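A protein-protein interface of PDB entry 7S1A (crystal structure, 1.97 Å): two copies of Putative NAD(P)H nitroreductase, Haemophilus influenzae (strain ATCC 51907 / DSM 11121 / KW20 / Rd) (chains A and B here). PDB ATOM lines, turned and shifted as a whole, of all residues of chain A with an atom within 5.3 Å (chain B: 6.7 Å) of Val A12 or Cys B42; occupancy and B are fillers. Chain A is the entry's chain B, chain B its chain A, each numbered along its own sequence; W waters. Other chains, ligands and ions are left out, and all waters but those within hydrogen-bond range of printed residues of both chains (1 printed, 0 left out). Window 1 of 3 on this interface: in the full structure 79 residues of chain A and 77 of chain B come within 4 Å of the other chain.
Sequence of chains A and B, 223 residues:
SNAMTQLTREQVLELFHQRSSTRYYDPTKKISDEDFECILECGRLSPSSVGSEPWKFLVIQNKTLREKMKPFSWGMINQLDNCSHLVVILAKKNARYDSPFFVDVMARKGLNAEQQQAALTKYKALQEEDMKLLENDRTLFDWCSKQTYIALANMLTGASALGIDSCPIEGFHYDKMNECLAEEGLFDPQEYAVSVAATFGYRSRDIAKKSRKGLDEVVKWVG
O of Gln A11 sits at hydrogen-bond distance from OG1 of Thr B5 (3.0 Å). N of Thr B5 lies within hydrogen-bond range of OE1 of Glu A14. The side-chain sulfur of Cys B38 lies within hydrogen-bond range of the backbone carbonyl oxygen of Arg A9 (3.7 Å). O of Ala B161 lies within hydrogen-bond range of N of Leu A7 (3.1 Å).
The backbone carbonyl oxygen (O) of Cys B38 lies within hydrogen-bond range of the side-chain sulfur (SG) of Cys B42 (3.4 Å). The guanidinium group of Arg B44 is in salt-bridge range of the side-chain carboxylate of Glu B41 (3.6 Å). The backbone carbonyl oxygen (O) of Cys B42 lies within hydrogen-bond range of the side-chain hydroxyl (OG) of Ser B46, at 2.9 Å. The side-chain amide nitrogen (ND2) of Asn B154 lies within hydrogen-bond range of the side-chain hydroxyl (OG) of Ser B46 (2.8 Å). O of Ile B150 sits at hydrogen-bond distance from ND2 of Asn B154 (3.4 Å). The side-chain hydroxyl (OG1) of Thr A8 is in hydrogen-bond range of the side-chain carboxylate (OE1) of Glu A10 (3.4 Å).
Leu A7 touches Leu B162. Thr A8 touches Leu B162 (O to CD2, 3.8 Å). CG1 of Val A12 touches SG of Cys B38, 3.6 Å away. CG1 of Val A12 touches SG of Cys B42 (3.7 Å). CG2 of Val A12 touches CB of Ala B161, 3.9 Å away. Leu B162 touches Val A12 (CD2 to CG2, 3.7 Å). Cys B38 touches Leu A13 (SG to CD2, 3.9 Å). Glu B41 touches Leu A13 (CG to CD2, 3.6 Å). Cys B42 touches Phe A16 (SG to CE2, 3.6 Å). Phe A16 touches Asn B154 (CE1 to CG, 3.4 Å).
Of the printed residues of chain B, Gln A11 touches Thr B5 (3.0 Å). Val A12 touches four residues of chain B. Of the printed residues of chain B, Leu A13 touches Cys B38 and Glu B41. Of the printed residues of chain B, Leu A15 touches Thr B5. Printed residues of chain B within 4 Å of Phe A16: Cys B42 and Asn B154. Of the printed residues of chain A, Cys B38 touches Arg A9, Val A12 and Leu A13. Cys B42 touches two residues of chain A. The nearest printed residue of chain B that does not touch Phe A16 is Leu B45 (4.1 Å).
Of the 10 printed residues of chain A, 9 touch a printed residue of chain B. Hydrophobic or aromatic side chains of chain A within 4 Å of the printed part of chain B: Val A12, Leu A13, Leu A15 and Phe A16. Hydrophobic or aromatic side chains of chain B that line the printed part of chain A: Ala B161 and Leu B162. Among the printed residues, no Asp or Glu carboxylate lies within 4 Å of a Lys or Arg side-chain nitrogen of the other chain.
No position is printed for both chains. Of the 15 pairs that touch across the chains among the printed residues, none has its exchanged pair printed and touching as well.
Water W1 lies within hydrogen-bond range of the backbone carbonyl oxygen of Phe A16 (3.0 Å) and the backbone carbonyl oxygen of Leu B45 (3.2 Å).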
ATOM      1  N   LEU A   7     -20.579   2.857   0.351  1.00  0.00           N
ATOM      2  CA  LEU A   7     -19.713   2.849   1.524  1.00  0.00           C
ATOM      3  C   LEU A   7     -19.632   1.430   2.072  1.00  0.00           C
ATOM      4  O   LEU A   7     -20.530   0.614   1.858  1.00  0.00           O
ATOM      5  CB  LEU A   7     -20.229   3.784   2.624  1.00  0.00           C
ATOM      6  CG  LEU A   7     -20.181   5.298   2.431  1.00  0.00           C
ATOM      7  CD1 LEU A   7     -20.818   5.995   3.623  1.00  0.00           C
ATOM      8  CD2 LEU A   7     -18.761   5.775   2.272  1.00  0.00           C
ATOM      9  N   THR A   8     -18.552   1.145   2.794  1.00  0.00           N
ATOM     10  CA  THR A   8     -18.429  -0.132   3.475  1.00  0.00           C
ATOM     11  C   THR A   8     -19.305  -0.134   4.725  1.00  0.00           C
ATOM     12  O   THR A   8     -19.926   0.868   5.090  1.00  0.00           O
ATOM     13  CB  THR A   8     -16.985  -0.414   3.883  1.00  0.00           C
ATOM     14  OG1 THR A   8     -16.591   0.542   4.875  1.00  0.00           O
ATOM     15  CG2 THR A   8     -16.039  -0.367   2.695  1.00  0.00           C
ATOM     16  N   ARG A   9     -19.355  -1.280   5.399  1.00  0.00           N
ATOM     17  CA  ARG A   9     -20.064  -1.332   6.672  1.00  0.00           C
ATOM     18  C   ARG A   9     -19.361  -0.482   7.720  1.00  0.00           C
ATOM     19  O   ARG A   9     -20.012   0.250   8.473  1.00  0.00           O
ATOM     20  CB  ARG A   9     -20.187  -2.776   7.149  1.00  0.00           C
ATOM     21  CG  ARG A   9     -21.228  -3.573   6.411  1.00  0.00           C
ATOM     22  CD  ARG A   9     -21.561  -4.809   7.189  1.00  0.00           C
ATOM     23  NE  ARG A   9     -20.380  -5.631   7.408  1.00  0.00           N
ATOM     24  CZ  ARG A   9     -19.992  -6.593   6.584  1.00  0.00           C
ATOM     25  NH1 ARG A   9     -20.658  -6.858   5.472  1.00  0.00           N
ATOM     26  NH2 ARG A   9     -18.921  -7.320   6.892  1.00  0.00           N
ATOM     27  N   GLU A  10     -18.028  -0.550   7.770  1.00  0.00           N
ATOM     28  CA  GLU A  10     -17.290   0.175   8.800  1.00  0.00           C
ATOM     29  C   GLU A  10     -17.430   1.679   8.622  1.00  0.00           C
ATOM     30  O   GLU A  10     -17.530   2.424   9.603  1.00  0.00           O
ATOM     31  CB  GLU A  10     -15.817  -0.230   8.777  1.00  0.00           C
ATOM     32  CG  GLU A  10     -15.563  -1.703   9.081  1.00  0.00           C
ATOM     33  CD  GLU A  10     -15.752  -2.602   7.867  1.00  0.00           C
ATOM     34  OE1 GLU A  10     -15.629  -2.106   6.724  1.00  0.00           O
ATOM     35  OE2 GLU A  10     -16.023  -3.809   8.057  1.00  0.00           O
ATOM     36  N   GLN A  11     -17.441   2.138   7.374  1.00  0.00           N
ATOM     37  CA  GLN A  11     -17.598   3.559   7.107  1.00  0.00           C
ATOM     38  C   GLN A  11     -19.003   4.027   7.444  1.00  0.00           C
ATOM     39  O   GLN A  11     -19.184   5.109   8.016  1.00  0.00           O
ATOM     40  CB  GLN A  11     -17.295   3.841   5.644  1.00  0.00           C
ATOM     41  CG  GLN A  11     -15.821   3.828   5.272  1.00  0.00           C
ATOM     42  CD  GLN A  11     -15.639   3.742   3.772  1.00  0.00           C
ATOM     43  OE1 GLN A  11     -16.613   3.559   3.041  1.00  0.00           O
ATOM     44  NE2 GLN A  11     -14.396   3.862   3.303  1.00  0.00           N
ATOM     45  N   VAL A  12     -20.009   3.240   7.063  1.00  0.00           N
ATOM     46  CA  VAL A  12     -21.388   3.573   7.409  1.00  0.00           C
ATOM     47  C   VAL A  12     -21.529   3.723   8.916  1.00  0.00           C
ATOM     48  O   VAL A  12     -22.112   4.695   9.407  1.00  0.00           O
ATOM     49  CB  VAL A  12     -22.345   2.515   6.836  1.00  0.00           C
ATOM     50  CG1 VAL A  12     -23.716   2.629   7.467  1.00  0.00           C
ATOM     51  CG2 VAL A  12     -22.426   2.666   5.313  1.00  0.00           C
ATOM     52  N   LEU A  13     -20.975   2.774   9.675  1.00  0.00           N
ATOM     53  CA  LEU A  13     -20.947   2.908  11.129  1.00  0.00           C
ATOM     54  C   LEU A  13     -20.261   4.197  11.558  1.00  0.00           C
ATOM     55  O   LEU A  13     -20.833   5.005  12.303  1.00  0.00           O
ATOM     56  CB  LEU A  13     -20.234   1.715  11.752  1.00  0.00           C
ATOM     57  CG  LEU A  13     -21.030   0.440  11.581  1.00  0.00           C
ATOM     58  CD1 LEU A  13     -20.363  -0.691  12.345  1.00  0.00           C
ATOM     59  CD2 LEU A  13     -22.450   0.690  12.053  1.00  0.00           C
ATOM     60  N   GLU A  14     -19.029   4.410  11.092  1.00  0.00           N
ATOM     61  CA  GLU A  14     -18.261   5.550  11.570  1.00  0.00           C
ATOM     62  C   GLU A  14     -18.947   6.864  11.227  1.00  0.00           C
ATOM     63  O   GLU A  14     -18.815   7.848  11.966  1.00  0.00           O
ATOM     64  CB  GLU A  14     -16.850   5.504  11.008  1.00  0.00           C
ATOM     65  CG  GLU A  14     -15.857   6.169  11.915  1.00  0.00           C
ATOM     66  CD  GLU A  14     -15.618   7.619  11.548  1.00  0.00           C
ATOM     67  OE1 GLU A  14     -15.425   7.907  10.343  1.00  0.00           O
ATOM     68  OE2 GLU A  14     -15.616   8.475  12.461  1.00  0.00           O
ATOM     69  N   LEU A  15     -19.724   6.885  10.145  1.00  0.00           N
ATOM     70  CA  LEU A  15     -20.495   8.076   9.801  1.00  0.00           C
ATOM     71  C   LEU A  15     -21.538   8.403  10.869  1.00  0.00           C
ATOM     72  O   LEU A  15     -21.760   9.577  11.202  1.00  0.00           O
ATOM     73  CB  LEU A  15     -21.147   7.872   8.435  1.00  0.00           C
ATOM     74  CG  LEU A  15     -22.203   8.871   8.000  1.00  0.00           C
ATOM     75  CD1 LEU A  15     -21.606  10.273   7.956  1.00  0.00           C
ATOM     76  CD2 LEU A  15     -22.742   8.468   6.656  1.00  0.00           C
ATOM     77  N   PHE A  16     -22.202   7.391  11.417  1.00  0.00           N
ATOM     78  CA  PHE A  16     -23.182   7.682  12.453  1.00  0.00           C
ATOM     79  C   PHE A  16     -22.555   7.808  13.836  1.00  0.00           C
ATOM     80  O   PHE A  16     -23.159   8.422  14.719  1.00  0.00           O
ATOM     81  CB  PHE A  16     -24.307   6.628  12.429  1.00  0.00           C
ATOM     82  CG  PHE A  16     -25.217   6.784  11.242  1.00  0.00           C
ATOM     83  CD1 PHE A  16     -26.261   7.704  11.272  1.00  0.00           C
ATOM     84  CD2 PHE A  16     -24.969   6.094  10.065  1.00  0.00           C
ATOM     85  CE1 PHE A  16     -27.070   7.894  10.165  1.00  0.00           C
ATOM     86  CE2 PHE A  16     -25.771   6.270   8.957  1.00  0.00           C
ATOM     87  CZ  PHE A  16     -26.819   7.164   8.998  1.00  0.00           C
ATOM     88  N   THR B   5     -15.071   9.268   7.846  1.00  0.00           N
ATOM     89  CA  THR B   5     -15.927   9.106   6.674  1.00  0.00           C
ATOM     90  C   THR B   5     -16.270  10.458   6.072  1.00  0.00           C
ATOM     91  O   THR B   5     -16.873  11.306   6.730  1.00  0.00           O
ATOM     92  CB  THR B   5     -17.233   8.358   7.010  1.00  0.00           C
ATOM     93  OG1 THR B   5     -16.932   7.002   7.360  1.00  0.00           O
ATOM     94  CG2 THR B   5     -18.174   8.364   5.816  1.00  0.00           C
ATOM     95  N   GLU B  37     -27.480  -5.938  10.258  1.00  0.00           N
ATOM     96  CA  GLU B  37     -27.077  -5.387  11.548  1.00  0.00           C
ATOM     97  C   GLU B  37     -26.553  -3.973  11.390  1.00  0.00           C
ATOM     98  O   GLU B  37     -26.819  -3.106  12.230  1.00  0.00           O
ATOM     99  CB  GLU B  37     -26.017  -6.258  12.210  1.00  0.00           C
ATOM    100  CG  GLU B  37     -25.539  -5.662  13.524  1.00  0.00           C
ATOM    101  CD  GLU B  37     -24.780  -6.651  14.382  1.00  0.00           C
ATOM    102  OE1 GLU B  37     -24.991  -7.874  14.213  1.00  0.00           O
ATOM    103  OE2 GLU B  37     -23.971  -6.201  15.223  1.00  0.00           O
ATOM    104  N   CYS B  38     -25.805  -3.714  10.313  1.00  0.00           N
ATOM    105  CA  CYS B  38     -25.321  -2.364  10.069  1.00  0.00           C
ATOM    106  C   CYS B  38     -26.485  -1.388   9.940  1.00  0.00           C
ATOM    107  O   CYS B  38     -26.511  -0.344  10.599  1.00  0.00           O
ATOM    108  CB  CYS B  38     -24.436  -2.344   8.825  1.00  0.00           C
ATOM    109  SG  CYS B  38     -23.555  -0.809   8.657  1.00  0.00           S
ATOM    110  N   ILE B  39     -27.498  -1.759   9.150  1.00  0.00           N
ATOM    111  CA  ILE B  39     -28.701  -0.935   9.006  1.00  0.00           C
ATOM    112  C   ILE B  39     -29.353  -0.678  10.361  1.00  0.00           C
ATOM    113  O   ILE B  39     -29.682   0.461  10.694  1.00  0.00           O
ATOM    114  CB  ILE B  39     -29.681  -1.599   8.023  1.00  0.00           C
ATOM    115  CG1 ILE B  39     -29.061  -1.649   6.623  1.00  0.00           C
ATOM    116  CG2 ILE B  39     -30.995  -0.861   7.974  1.00  0.00           C
ATOM    117  CD1 ILE B  39     -29.818  -2.571   5.685  1.00  0.00           C
ATOM    118  N   LEU B  40     -29.568  -1.734  11.155  1.00  0.00           N
ATOM    119  CA  LEU B  40     -30.145  -1.554  12.491  1.00  0.00           C
ATOM    120  C   LEU B  40     -29.333  -0.567  13.323  1.00  0.00           C
ATOM    121  O   LEU B  40     -29.893   0.305  13.996  1.00  0.00           O
ATOM    122  CB  LEU B  40     -30.230  -2.897  13.217  1.00  0.00           C
ATOM    123  CG  LEU B  40     -31.243  -3.913  12.699  1.00  0.00           C
ATOM    124  CD1 LEU B  40     -31.052  -5.292  13.363  1.00  0.00           C
ATOM    125  CD2 LEU B  40     -32.665  -3.416  12.882  1.00  0.00           C
ATOM    126  N   GLU B  41     -28.008  -0.700  13.289  1.00  0.00           N
ATOM    127  CA  GLU B  41     -27.126   0.209  14.014  1.00  0.00           C
ATOM    128  C   GLU B  41     -27.377   1.671  13.648  1.00  0.00           C
ATOM    129  O   GLU B  41     -27.236   2.567  14.492  1.00  0.00           O
ATOM    130  CB  GLU B  41     -25.678  -0.171  13.712  1.00  0.00           C
ATOM    131  CG  GLU B  41     -24.710   0.194  14.796  1.00  0.00           C
ATOM    132  CD  GLU B  41     -24.512  -0.936  15.762  1.00  0.00           C
ATOM    133  OE1 GLU B  41     -25.489  -1.654  16.028  1.00  0.00           O
ATOM    134  OE2 GLU B  41     -23.375  -1.121  16.242  1.00  0.00           O
ATOM    135  N   CYS B  42     -27.695   1.942  12.380  1.00  0.00           N
ATOM    136  CA  CYS B  42     -27.990   3.316  11.981  1.00  0.00           C
ATOM    137  C   CYS B  42     -29.191   3.872  12.747  1.00  0.00           C
ATOM    138  O   CYS B  42     -29.197   5.038  13.149  1.00  0.00           O
ATOM    139  CB  CYS B  42     -28.224   3.366  10.476  1.00  0.00           C
ATOM    140  SG  CYS B  42     -26.761   2.869   9.563  1.00  0.00           S
ATOM    141  N   GLY B  43     -30.218   3.058  12.968  1.00  0.00           N
ATOM    142  CA  GLY B  43     -31.304   3.512  13.822  1.00  0.00           C
ATOM    143  C   GLY B  43     -30.852   3.705  15.254  1.00  0.00           C
ATOM    144  O   GLY B  43     -31.087   4.753  15.860  1.00  0.00           O
ATOM    145  N   ARG B  44     -30.159   2.711  15.802  1.00  0.00           N
ATOM    146  CA  ARG B  44     -29.816   2.736  17.223  1.00  0.00           C
ATOM    147  C   ARG B  44     -28.915   3.919  17.583  1.00  0.00           C
ATOM    148  O   ARG B  44     -29.034   4.493  18.681  1.00  0.00           O
ATOM    149  CB  ARG B  44     -29.167   1.405  17.578  1.00  0.00           C
ATOM    150  CG  ARG B  44     -28.575   1.310  18.948  1.00  0.00           C
ATOM    151  CD  ARG B  44     -27.488   0.222  18.971  1.00  0.00           C
ATOM    152  NE  ARG B  44     -26.664   0.441  20.151  1.00  0.00           N
ATOM    153  CZ  ARG B  44     -25.383   0.776  20.148  1.00  0.00           C
ATOM    154  NH1 ARG B  44     -24.652   0.725  19.043  1.00  0.00           N
ATOM    155  NH2 ARG B  44     -24.814   1.162  21.289  1.00  0.00           N
ATOM    156  N   LEU B  45     -28.024   4.311  16.673  1.00  0.00           N
ATOM    157  CA  LEU B  45     -27.114   5.438  16.858  1.00  0.00           C
ATOM    158  C   LEU B  45     -27.756   6.787  16.546  1.00  0.00           C
ATOM    159  O   LEU B  45     -27.088   7.822  16.687  1.00  0.00           O
ATOM    160  CB  LEU B  45     -25.872   5.252  15.983  1.00  0.00           C
ATOM    161  CG  LEU B  45     -24.952   4.115  16.425  1.00  0.00           C
ATOM    162  CD1 LEU B  45     -23.805   3.873  15.421  1.00  0.00           C
ATOM    163  CD2 LEU B  45     -24.404   4.417  17.804  1.00  0.00           C
ATOM    164  N   SER B  46     -29.028   6.807  16.153  1.00  0.00           N
ATOM    165  CA  SER B  46     -29.685   8.057  15.798  1.00  0.00           C
ATOM    166  C   SER B  46     -29.811   8.988  16.999  1.00  0.00           C
ATOM    167  O   SER B  46     -29.929   8.548  18.149  1.00  0.00           O
ATOM    168  CB  SER B  46     -31.071   7.788  15.202  1.00  0.00           C
ATOM    169  OG  SER B  46     -30.941   7.256  13.880  1.00  0.00           O
ATOM    170  N   PRO B  47     -29.804  10.288  16.755  1.00  0.00           N
ATOM    171  CA  PRO B  47     -30.084  11.241  17.830  1.00  0.00           C
ATOM    172  C   PRO B  47     -31.560  11.228  18.179  1.00  0.00           C
ATOM    173  O   PRO B  47     -32.398  10.818  17.383  1.00  0.00           O
ATOM    174  CB  PRO B  47     -29.683  12.583  17.218  1.00  0.00           C
ATOM    175  CG  PRO B  47     -29.949  12.381  15.765  1.00  0.00           C
ATOM    176  CD  PRO B  47     -29.603  10.955  15.459  1.00  0.00           C
ATOM    177  N   PHE B  57     -37.212  -1.714  17.583  1.00  0.00           N
ATOM    178  CA  PHE B  57     -37.184  -2.189  16.199  1.00  0.00           C
ATOM    179  C   PHE B  57     -37.611  -3.642  16.181  1.00  0.00           C
ATOM    180  O   PHE B  57     -36.841  -4.527  16.566  1.00  0.00           O
ATOM    181  CB  PHE B  57     -35.797  -2.004  15.570  1.00  0.00           C
ATOM    182  CG  PHE B  57     -35.271  -0.620  15.705  1.00  0.00           C
ATOM    183  CD1 PHE B  57     -36.049   0.475  15.332  1.00  0.00           C
ATOM    184  CD2 PHE B  57     -34.012  -0.392  16.236  1.00  0.00           C
ATOM    185  CE1 PHE B  57     -35.565   1.779  15.473  1.00  0.00           C
ATOM    186  CE2 PHE B  57     -33.528   0.885  16.368  1.00  0.00           C
ATOM    187  CZ  PHE B  57     -34.309   1.984  15.999  1.00  0.00           C
ATOM    188  N   ILE B 150     -36.576   9.716  12.865  1.00  0.00           N
ATOM    189  CA  ILE B 150     -35.156   9.954  12.638  1.00  0.00           C
ATOM    190  C   ILE B 150     -34.436   8.630  12.428  1.00  0.00           C
ATOM    191  O   ILE B 150     -33.659   8.466  11.475  1.00  0.00           O
ATOM    192  CB  ILE B 150     -34.553  10.750  13.811  1.00  0.00           C
ATOM    193  CG1 ILE B 150     -35.249  12.090  13.961  1.00  0.00           C
ATOM    194  CG2 ILE B 150     -33.095  10.980  13.576  1.00  0.00           C
ATOM    195  CD1 ILE B 150     -34.748  12.904  15.136  1.00  0.00           C
ATOM    196  N   ALA B 151     -34.719   7.644  13.289  1.00  0.00           N
ATOM    197  CA  ALA B 151     -34.145   6.321  13.090  1.00  0.00           C
ATOM    198  C   ALA B 151     -34.606   5.733  11.768  1.00  0.00           C
ATOM    199  O   ALA B 151     -33.837   5.047  11.085  1.00  0.00           O
ATOM    200  CB  ALA B 151     -34.511   5.401  14.251  1.00  0.00           C
ATOM    201  N   ASN B 154     -32.489   7.409   8.928  1.00  0.00           N
ATOM    202  CA  ASN B 154     -31.090   7.013   8.898  1.00  0.00           C
ATOM    203  C   ASN B 154     -30.927   5.570   8.484  1.00  0.00           C
ATOM    204  O   ASN B 154     -29.908   5.214   7.893  1.00  0.00           O
ATOM    205  CB  ASN B 154     -30.443   7.248  10.250  1.00  0.00           C
ATOM    206  CG  ASN B 154     -30.296   8.709  10.561  1.00  0.00           C
ATOM    207  OD1 ASN B 154     -30.127   9.537   9.663  1.00  0.00           O
ATOM    208  ND2 ASN B 154     -30.329   9.040  11.820  1.00  0.00           N
ATOM    209  N   MET B 155     -31.906   4.729   8.782  1.00  0.00           N
ATOM    210  CA  MET B 155     -31.839   3.369   8.324  1.00  0.00           C
ATOM    211  C   MET B 155     -32.005   3.325   6.808  1.00  0.00           C
ATOM    212  O   MET B 155     -31.336   2.550   6.130  1.00  0.00           O
ATOM    213  CB  MET B 155     -32.890   2.509   9.045  1.00  0.00           C
ATOM    214  CG  MET B 155     -32.443   2.132  10.456  1.00  0.00           C
ATOM    215  SD  MET B 155     -33.667   0.912  11.402  1.00  0.00           S
ATOM    216  CE  MET B 155     -35.107   2.181  11.672  1.00  0.00           C
ATOM    217  N   LEU B 156     -32.890   4.151   6.253  1.00  0.00           N
ATOM    218  CA  LEU B 156     -32.976   4.200   4.796  1.00  0.00           C
ATOM    219  C   LEU B 156     -31.650   4.655   4.199  1.00  0.00           C
ATOM    220  O   LEU B 156     -31.126   4.052   3.244  1.00  0.00           O
ATOM    221  CB  LEU B 156     -34.106   5.132   4.364  1.00  0.00           C
ATOM    222  CG  LEU B 156     -35.478   4.960   4.994  1.00  0.00           C
ATOM    223  CD1 LEU B 156     -36.362   6.035   4.427  1.00  0.00           C
ATOM    224  CD2 LEU B 156     -36.053   3.570   4.682  1.00  0.00           C
ATOM    225  N   THR B 157     -31.068   5.709   4.771  1.00  0.00           N
ATOM    226  CA  THR B 157     -29.858   6.259   4.171  1.00  0.00           C
ATOM    227  C   THR B 157     -28.701   5.284   4.312  1.00  0.00           C
ATOM    228  O   THR B 157     -28.000   4.985   3.332  1.00  0.00           O
ATOM    229  CB  THR B 157     -29.535   7.606   4.795  1.00  0.00           C
ATOM    230  OG1 THR B 157     -30.644   8.473   4.568  1.00  0.00           O
ATOM    231  CG2 THR B 157     -28.325   8.210   4.112  1.00  0.00           C
ATOM    232  N   GLY B 158     -28.528   4.724   5.516  1.00  0.00           N
ATOM    233  CA  GLY B 158     -27.523   3.685   5.699  1.00  0.00           C
ATOM    234  C   GLY B 158     -27.724   2.512   4.759  1.00  0.00           C
ATOM    235  O   GLY B 158     -26.769   2.017   4.149  1.00  0.00           O
ATOM    236  N   ALA B 159     -28.970   2.048   4.624  1.00  0.00           N
ATOM    237  CA  ALA B 159     -29.251   0.986   3.665  1.00  0.00           C
ATOM    238  C   ALA B 159     -28.805   1.391   2.263  1.00  0.00           C
ATOM    239  O   ALA B 159     -28.046   0.672   1.594  1.00  0.00           O
ATOM    240  CB  ALA B 159     -30.740   0.653   3.685  1.00  0.00           C
ATOM    241  N   ALA B 161     -26.599   3.470   1.379  1.00  0.00           N
ATOM    242  CA  ALA B 161     -25.150   3.533   1.255  1.00  0.00           C
ATOM    243  C   ALA B 161     -24.542   2.147   1.073  1.00  0.00           C
ATOM    244  O   ALA B 161     -23.509   2.011   0.406  1.00  0.00           O
ATOM    245  CB  ALA B 161     -24.542   4.244   2.469  1.00  0.00           C
ATOM    246  N   LEU B 162     -25.172   1.110   1.619  1.00  0.00           N
ATOM    247  CA  LEU B 162     -24.661  -0.248   1.461  1.00  0.00           C
ATOM    248  C   LEU B 162     -25.095  -0.896   0.156  1.00  0.00           C
ATOM    249  O   LEU B 162     -24.811  -2.078  -0.048  1.00  0.00           O
ATOM    250  CB  LEU B 162     -25.109  -1.140   2.629  1.00  0.00           C
ATOM    251  CG  LEU B 162     -24.731  -0.765   4.067  1.00  0.00           C
ATOM    252  CD1 LEU B 162     -25.408  -1.713   5.056  1.00  0.00           C
ATOM    253  CD2 LEU B 162     -23.228  -0.763   4.273  1.00  0.00           C
HETATM  254  O   HOH W   1     -25.849   9.695  14.424  1.00  0.00           O
